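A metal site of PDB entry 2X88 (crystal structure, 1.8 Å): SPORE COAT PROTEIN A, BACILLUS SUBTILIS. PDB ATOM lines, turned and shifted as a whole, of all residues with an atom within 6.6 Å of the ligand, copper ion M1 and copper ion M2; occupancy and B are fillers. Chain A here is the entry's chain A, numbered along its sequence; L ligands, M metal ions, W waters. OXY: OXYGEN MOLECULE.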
ATOM      1  N   HIS A 105      23.055   2.696  24.620  1.00  0.00           N
ATOM      2  CA  HIS A 105      22.862   1.311  24.195  1.00  0.00           C
ATOM      3  C   HIS A 105      23.347   1.122  22.761  1.00  0.00           C
ATOM      4  O   HIS A 105      22.915   1.852  21.863  1.00  0.00           O
ATOM      5  CB  HIS A 105      21.387   0.904  24.320  1.00  0.00           C
ATOM      6  CG  HIS A 105      21.066  -0.416  23.680  1.00  0.00           C
ATOM      7  ND1 HIS A 105      21.697  -1.587  24.041  1.00  0.00           N
ATOM      8  CD2 HIS A 105      20.183  -0.746  22.714  1.00  0.00           C
ATOM      9  CE1 HIS A 105      21.209  -2.587  23.315  1.00  0.00           C
ATOM     10  NE2 HIS A 105      20.294  -2.103  22.507  1.00  0.00           N
ATOM     11  N   LEU A 106      24.227   0.151  22.563  1.00  0.00           N
ATOM     12  CA  LEU A 106      24.612  -0.246  21.219  1.00  0.00           C
ATOM     13  C   LEU A 106      23.599  -1.284  20.717  1.00  0.00           C
ATOM     14  O   LEU A 106      23.664  -2.457  21.081  1.00  0.00           O
ATOM     15  CB  LEU A 106      26.045  -0.808  21.191  1.00  0.00           C
ATOM     16  CG  LEU A 106      26.553  -1.295  19.815  1.00  0.00           C
ATOM     17  CD1 LEU A 106      26.454  -0.188  18.765  1.00  0.00           C
ATOM     18  CD2 LEU A 106      27.980  -1.826  19.917  1.00  0.00           C
ATOM     19  N   HIS A 107      22.667  -0.812  19.895  1.00  0.00           N
ATOM     20  CA  HIS A 107      21.585  -1.632  19.364  1.00  0.00           C
ATOM     21  C   HIS A 107      22.123  -2.693  18.406  1.00  0.00           C
ATOM     22  O   HIS A 107      22.723  -2.364  17.373  1.00  0.00           O
ATOM     23  CB  HIS A 107      20.528  -0.763  18.668  1.00  0.00           C
ATOM     24  CG  HIS A 107      19.291  -1.505  18.276  1.00  0.00           C
ATOM     25  ND1 HIS A 107      18.043  -1.185  18.758  1.00  0.00           N
ATOM     26  CD2 HIS A 107      19.116  -2.554  17.437  1.00  0.00           C
ATOM     27  CE1 HIS A 107      17.149  -2.010  18.244  1.00  0.00           C
ATOM     28  NE2 HIS A 107      17.772  -2.847  17.439  1.00  0.00           N
ATOM     29  N   GLY A 108      21.912  -3.958  18.751  1.00  0.00           N
ATOM     30  CA  GLY A 108      22.443  -5.093  17.995  1.00  0.00           C
ATOM     31  C   GLY A 108      23.766  -5.609  18.526  1.00  0.00           C
ATOM     32  O   GLY A 108      24.276  -6.629  18.064  1.00  0.00           O
ATOM     33  N   GLY A 117      23.959  -0.913  28.262  1.00  0.00           N
ATOM     34  CA  GLY A 117      23.144   0.289  28.411  1.00  0.00           C
ATOM     35  C   GLY A 117      21.767  -0.004  28.985  1.00  0.00           C
ATOM     36  O   GLY A 117      20.755   0.453  28.446  1.00  0.00           O
ATOM     37  N   PRO A 119      18.480   0.300  31.111  1.00  0.00           N
ATOM     38  CA  PRO A 119      17.774   1.560  31.385  1.00  0.00           C
ATOM     39  C   PRO A 119      18.036   2.119  32.782  1.00  0.00           C
ATOM     40  O   PRO A 119      18.048   3.335  32.962  1.00  0.00           O
ATOM     41  CB  PRO A 119      16.296   1.180  31.227  1.00  0.00           C
ATOM     42  CG  PRO A 119      16.293  -0.049  30.398  1.00  0.00           C
ATOM     43  CD  PRO A 119      17.550  -0.775  30.748  1.00  0.00           C
ATOM     44  N   TRP A 151      23.452   0.436  15.521  1.00  0.00           N
ATOM     45  CA  TRP A 151      23.325   1.860  15.820  1.00  0.00           C
ATOM     46  C   TRP A 151      23.293   2.067  17.314  1.00  0.00           C
ATOM     47  O   TRP A 151      22.925   1.161  18.070  1.00  0.00           O
ATOM     48  CB  TRP A 151      22.126   2.501  15.090  1.00  0.00           C
ATOM     49  CG  TRP A 151      20.742   2.063  15.501  1.00  0.00           C
ATOM     50  CD1 TRP A 151      20.201   0.810  15.409  1.00  0.00           C
ATOM     51  CD2 TRP A 151      19.700   2.914  16.023  1.00  0.00           C
ATOM     52  NE1 TRP A 151      18.901   0.819  15.869  1.00  0.00           N
ATOM     53  CE2 TRP A 151      18.571   2.101  16.246  1.00  0.00           C
ATOM     54  CE3 TRP A 151      19.630   4.282  16.332  1.00  0.00           C
ATOM     55  CZ2 TRP A 151      17.375   2.604  16.764  1.00  0.00           C
ATOM     56  CZ3 TRP A 151      18.435   4.785  16.850  1.00  0.00           C
ATOM     57  CH2 TRP A 151      17.320   3.949  17.058  1.00  0.00           C
ATOM     58  N   HIS A 153      22.229   4.630  20.671  1.00  0.00           N
ATOM     59  CA  HIS A 153      21.270   5.642  21.083  1.00  0.00           C
ATOM     60  C   HIS A 153      21.037   5.611  22.582  1.00  0.00           C
ATOM     61  O   HIS A 153      21.375   4.633  23.254  1.00  0.00           O
ATOM     62  CB  HIS A 153      19.930   5.487  20.326  1.00  0.00           C
ATOM     63  CG  HIS A 153      19.220   4.191  20.601  1.00  0.00           C
ATOM     64  ND1 HIS A 153      18.460   3.986  21.736  1.00  0.00           N
ATOM     65  CD2 HIS A 153      19.142   3.046  19.879  1.00  0.00           C
ATOM     66  CE1 HIS A 153      17.951   2.766  21.701  1.00  0.00           C
ATOM     67  NE2 HIS A 153      18.347   2.177  20.586  1.00  0.00           N
ATOM     68  N   ASP A 154      20.452   6.682  23.113  1.00  0.00           N
ATOM     69  CA  ASP A 154      20.155   6.742  24.545  1.00  0.00           C
ATOM     70  C   ASP A 154      19.088   5.728  24.939  1.00  0.00           C
ATOM     71  O   ASP A 154      18.192   5.419  24.144  1.00  0.00           O
ATOM     72  CB  ASP A 154      19.712   8.143  24.954  1.00  0.00           C
ATOM     73  CG  ASP A 154      19.684   8.308  26.454  1.00  0.00           C
ATOM     74  OD1 ASP A 154      18.585   8.206  27.037  1.00  0.00           O
ATOM     75  OD2 ASP A 154      20.757   8.490  27.048  1.00  0.00           O
ATOM     76  N   HIS A 155      19.181   5.225  26.164  1.00  0.00           N
ATOM     77  CA  HIS A 155      18.259   4.196  26.638  1.00  0.00           C
ATOM     78  C   HIS A 155      17.820   4.423  28.100  1.00  0.00           C
ATOM     79  O   HIS A 155      17.376   3.482  28.768  1.00  0.00           O
ATOM     80  CB  HIS A 155      18.918   2.810  26.489  1.00  0.00           C
ATOM     81  CG  HIS A 155      17.947   1.710  26.190  1.00  0.00           C
ATOM     82  ND1 HIS A 155      16.856   1.431  27.001  1.00  0.00           N
ATOM     83  CD2 HIS A 155      17.901   0.804  25.183  1.00  0.00           C
ATOM     84  CE1 HIS A 155      16.188   0.410  26.491  1.00  0.00           C
ATOM     85  NE2 HIS A 155      16.802   0.007  25.391  1.00  0.00           N
ATOM     86  N   THR A 160      13.751   7.702  27.332  1.00  0.00           N
ATOM     87  CA  THR A 160      14.290   7.272  26.040  1.00  0.00           C
ATOM     88  C   THR A 160      13.651   8.020  24.860  1.00  0.00           C
ATOM     89  O   THR A 160      14.363   8.479  23.956  1.00  0.00           O
ATOM     90  CB  THR A 160      14.209   5.728  25.886  1.00  0.00           C
ATOM     91  OG1 THR A 160      14.991   5.124  26.932  1.00  0.00           O
ATOM     92  CG2 THR A 160      14.758   5.271  24.538  1.00  0.00           C
ATOM     93  N   ALA A 297      13.944   1.168  14.512  1.00  0.00           N
ATOM     94  CA  ALA A 297      15.109   0.347  14.879  1.00  0.00           C
ATOM     95  C   ALA A 297      15.499  -0.750  13.886  1.00  0.00           C
ATOM     96  O   ALA A 297      16.576  -1.333  14.010  1.00  0.00           O
ATOM     97  CB  ALA A 297      14.984  -0.236  16.295  1.00  0.00           C
ATOM     98  N   HIS A 422      11.784  -5.841  19.976  1.00  0.00           N
ATOM     99  CA  HIS A 422      13.235  -5.943  19.990  1.00  0.00           C
ATOM    100  C   HIS A 422      13.729  -6.723  21.209  1.00  0.00           C
ATOM    101  O   HIS A 422      13.267  -6.486  22.333  1.00  0.00           O
ATOM    102  CB  HIS A 422      13.845  -4.541  19.949  1.00  0.00           C
ATOM    103  CG  HIS A 422      15.332  -4.520  20.104  1.00  0.00           C
ATOM    104  ND1 HIS A 422      16.180  -5.251  19.304  1.00  0.00           N
ATOM    105  CD2 HIS A 422      16.130  -3.840  20.961  1.00  0.00           C
ATOM    106  CE1 HIS A 422      17.423  -5.038  19.657  1.00  0.00           C
ATOM    107  NE2 HIS A 422      17.431  -4.179  20.670  1.00  0.00           N
ATOM    108  N   HIS A 424      17.334  -7.580  23.231  1.00  0.00           N
ATOM    109  CA  HIS A 424      18.758  -7.272  23.382  1.00  0.00           C
ATOM    110  C   HIS A 424      19.637  -8.510  23.232  1.00  0.00           C
ATOM    111  O   HIS A 424      19.137  -9.645  23.294  1.00  0.00           O
ATOM    112  CB  HIS A 424      19.015  -6.592  24.724  1.00  0.00           C
ATOM    113  CG  HIS A 424      18.600  -5.155  24.774  1.00  0.00           C
ATOM    114  ND1 HIS A 424      19.308  -4.206  25.467  1.00  0.00           N
ATOM    115  CD2 HIS A 424      17.557  -4.507  24.186  1.00  0.00           C
ATOM    116  CE1 HIS A 424      18.711  -3.030  25.332  1.00  0.00           C
ATOM    117  NE2 HIS A 424      17.656  -3.184  24.553  1.00  0.00           N
ATOM    118  N   THR A 466      14.954  -6.757  15.532  1.00  0.00           N
ATOM    119  CA  THR A 466      13.738  -5.971  15.715  1.00  0.00           C
ATOM    120  C   THR A 466      12.734  -6.428  14.659  1.00  0.00           C
ATOM    121  O   THR A 466      13.018  -6.386  13.462  1.00  0.00           O
ATOM    122  CB  THR A 466      14.028  -4.447  15.581  1.00  0.00           C
ATOM    123  OG1 THR A 466      15.073  -4.083  16.492  1.00  0.00           O
ATOM    124  CG2 THR A 466      12.777  -3.620  15.887  1.00  0.00           C
ATOM    125  N   VAL A 489      17.232  -6.812  28.360  1.00  0.00           N
ATOM    126  CA  VAL A 489      15.833  -6.401  28.245  1.00  0.00           C
ATOM    127  C   VAL A 489      15.242  -6.791  26.892  1.00  0.00           C
ATOM    128  O   VAL A 489      15.950  -7.154  25.958  1.00  0.00           O
ATOM    129  CB  VAL A 489      15.597  -4.864  28.465  1.00  0.00           C
ATOM    130  CG1 VAL A 489      16.048  -4.421  29.849  1.00  0.00           C
ATOM    131  CG2 VAL A 489      16.281  -4.041  27.392  1.00  0.00           C
ATOM    132  N   TRP A 490      13.918  -6.768  26.826  1.00  0.00           N
ATOM    133  CA  TRP A 490      13.185  -6.897  25.566  1.00  0.00           C
ATOM    134  C   TRP A 490      12.004  -5.937  25.617  1.00  0.00           C
ATOM    135  O   TRP A 490      11.459  -5.672  26.696  1.00  0.00           O
ATOM    136  CB  TRP A 490      12.764  -8.348  25.276  1.00  0.00           C
ATOM    137  CG  TRP A 490      11.606  -8.865  26.084  1.00  0.00           C
ATOM    138  CD1 TRP A 490      11.618  -9.252  27.391  1.00  0.00           C
ATOM    139  CD2 TRP A 490      10.271  -9.098  25.606  1.00  0.00           C
ATOM    140  NE1 TRP A 490      10.366  -9.686  27.772  1.00  0.00           N
ATOM    141  CE2 TRP A 490       9.524  -9.610  26.692  1.00  0.00           C
ATOM    142  CE3 TRP A 490       9.634  -8.911  24.369  1.00  0.00           C
ATOM    143  CZ2 TRP A 490       8.167  -9.934  26.580  1.00  0.00           C
ATOM    144  CZ3 TRP A 490       8.284  -9.241  24.259  1.00  0.00           C
ATOM    145  CH2 TRP A 490       7.562  -9.748  25.362  1.00  0.00           C
ATOM    146  N   HIS A 491      11.630  -5.378  24.460  1.00  0.00           N
ATOM    147  CA  HIS A 491      10.627  -4.307  24.430  1.00  0.00           C
ATOM    148  C   HIS A 491      10.123  -3.982  23.037  1.00  0.00           C
ATOM    149  O   HIS A 491      10.729  -4.374  22.028  1.00  0.00           O
ATOM    150  CB  HIS A 491      11.189  -3.030  25.074  1.00  0.00           C
ATOM    151  CG  HIS A 491      12.412  -2.487  24.405  1.00  0.00           C
ATOM    152  ND1 HIS A 491      12.359  -1.508  23.431  1.00  0.00           N
ATOM    153  CD2 HIS A 491      13.722  -2.785  24.578  1.00  0.00           C
ATOM    154  CE1 HIS A 491      13.588  -1.231  23.029  1.00  0.00           C
ATOM    155  NE2 HIS A 491      14.426  -1.984  23.711  1.00  0.00           N
ATOM    156  N   HIS A 493       9.929  -1.172  20.277  1.00  0.00           N
ATOM    157  CA  HIS A 493      10.855  -0.085  19.965  1.00  0.00           C
ATOM    158  C   HIS A 493      10.146   1.184  19.439  1.00  0.00           C
ATOM    159  O   HIS A 493      10.797   2.096  18.910  1.00  0.00           O
ATOM    160  CB  HIS A 493      11.958  -0.542  19.004  1.00  0.00           C
ATOM    161  CG  HIS A 493      13.290   0.117  19.231  1.00  0.00           C
ATOM    162  ND1 HIS A 493      13.498   1.461  19.002  1.00  0.00           N
ATOM    163  CD2 HIS A 493      14.465  -0.379  19.661  1.00  0.00           C
ATOM    164  CE1 HIS A 493      14.751   1.760  19.287  1.00  0.00           C
ATOM    165  NE2 HIS A 493      15.362   0.663  19.687  1.00  0.00           N
ATOM    166  N   LEU A 495       9.154   4.251  20.877  1.00  0.00           N
ATOM    167  CA  LEU A 495       9.722   4.781  22.117  1.00  0.00           C
ATOM    168  C   LEU A 495       8.662   5.280  23.084  1.00  0.00           C
ATOM    169  O   LEU A 495       8.837   5.180  24.299  1.00  0.00           O
ATOM    170  CB  LEU A 495      10.771   5.862  21.815  1.00  0.00           C
ATOM    171  CG  LEU A 495      11.937   5.441  20.908  1.00  0.00           C
ATOM    172  CD1 LEU A 495      12.963   6.557  20.835  1.00  0.00           C
ATOM    173  CD2 LEU A 495      12.605   4.145  21.374  1.00  0.00           C
ATOM    174  N   GLU A 498       7.598   2.024  24.712  1.00  0.00           N
ATOM    175  CA  GLU A 498       8.692   1.553  25.564  1.00  0.00           C
ATOM    176  C   GLU A 498       8.707   2.250  26.927  1.00  0.00           C
ATOM    177  O   GLU A 498       8.867   1.600  27.956  1.00  0.00           O
ATOM    178  CB  GLU A 498      10.030   1.751  24.845  1.00  0.00           C
ATOM    179  CG  GLU A 498      11.273   1.384  25.651  1.00  0.00           C
ATOM    180  CD  GLU A 498      12.550   1.609  24.862  1.00  0.00           C
ATOM    181  OE1 GLU A 498      12.490   1.639  23.610  1.00  0.00           O
ATOM    182  OE2 GLU A 498      13.615   1.744  25.489  1.00  0.00           O
ATOM    183  N   MET A 503       8.150  -2.624  28.195  1.00  0.00           N
ATOM    184  CA  MET A 503       9.537  -3.063  28.319  1.00  0.00           C
ATOM    185  C   MET A 503       9.669  -3.948  29.551  1.00  0.00           C
ATOM    186  O   MET A 503       9.098  -3.648  30.600  1.00  0.00           O
ATOM    187  CB  MET A 503      10.459  -1.848  28.438  1.00  0.00           C
ATOM    188  CG  MET A 503      11.934  -2.191  28.565  1.00  0.00           C
ATOM    189  SD  MET A 503      13.057  -0.792  28.436  1.00  0.00           S
ATOM    190  CE  MET A 503      12.631   0.141  29.902  1.00  0.00           C
HETATM  191  O1  OXY L   1      16.525  -0.150  22.415  1.00  0.00           O
HETATM  192  O2  OXY L   1      17.255  -0.946  21.934  1.00  0.00           O
HETATM  193 CU    CU M   1      17.487   0.427  19.884  1.00  0.00          CU
HETATM  194 CU    CU M   2      16.413  -1.633  24.124  1.00  0.00          CU
HETATM  195 CU    CU M   3      18.826  -3.100  21.575  1.00  0.00          CU
HETATM  196  O   HOH W   1      15.137   1.780  23.040  1.00  0.00           O
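Residues that only touch copper ion M1: Trp 151 (3.8 Å).
CD2 of His 422 touches copper ion M2, at 3.9 Å. Within 4 Å of copper ion M2: His 155, His 422, His 424 and His 491.
A ring nitrogen (NE2) of His 105 lies close to an oxygen (O2) of the ligand, at 3.3 Å. A ring nitrogen (NE2) of His 422 sits close to an oxygen (O2) of the ligand, at 3.5 Å. Eight residues have an atom within 4 Å of the ligand: His 105, His 107, His 153, His 155, His 422, His 424, His 491 and His 493. The nearest printed residue that does not touch the ligand is Glu 498 (4.6 Å).
ND1 of His 107 binds copper ion M1, 2.0 Å away. A ring nitrogen (NE2) of His 153 binds copper ion M1. Copper ion M1 is bound by NE2 of His 493, at 2.1 Å. Copper ion M1 is bound by an oxygen (O2) of the ligand (2.5 Å). Copper ion M1 has four donor atoms within binding distance.
OG1 of Thr 466 sits at hydrogen-bond distance from ND1 of His 422, at 3.2 Å. NE2 of His 107 lies within hydrogen-bond range of OG1 of Thr 466, at 3.1 Å. ND1 of His 422 lies close to NE2 of His 107, 3.4 Å away. ND1 of His 491 sits close to OE1 of Glu 498 (3.2 Å). O of Val 489 sits at hydrogen-bond distance from N of His 424. The side-chain hydroxyl (OG1) of Thr 160 sits close to the backbone carbonyl oxygen (O) of His 155 (3.4 Å). O of His 153 lies within hydrogen-bond range of N of His 105 (2.9 Å). O of Trp 151 sits at hydrogen-bond distance from N of His 107 (2.7 Å).
Copper ion M2 is bound by a ring nitrogen (NE2) of His 424 (2.0 Å), a ring nitrogen (NE2) of His 491 (2.1 Å), a ring nitrogen (NE2) of His 155 (2.1 Å) and an oxygen (O1) of the ligand (2.3 Å). Copper ion M2 has four donor atoms within binding distance.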
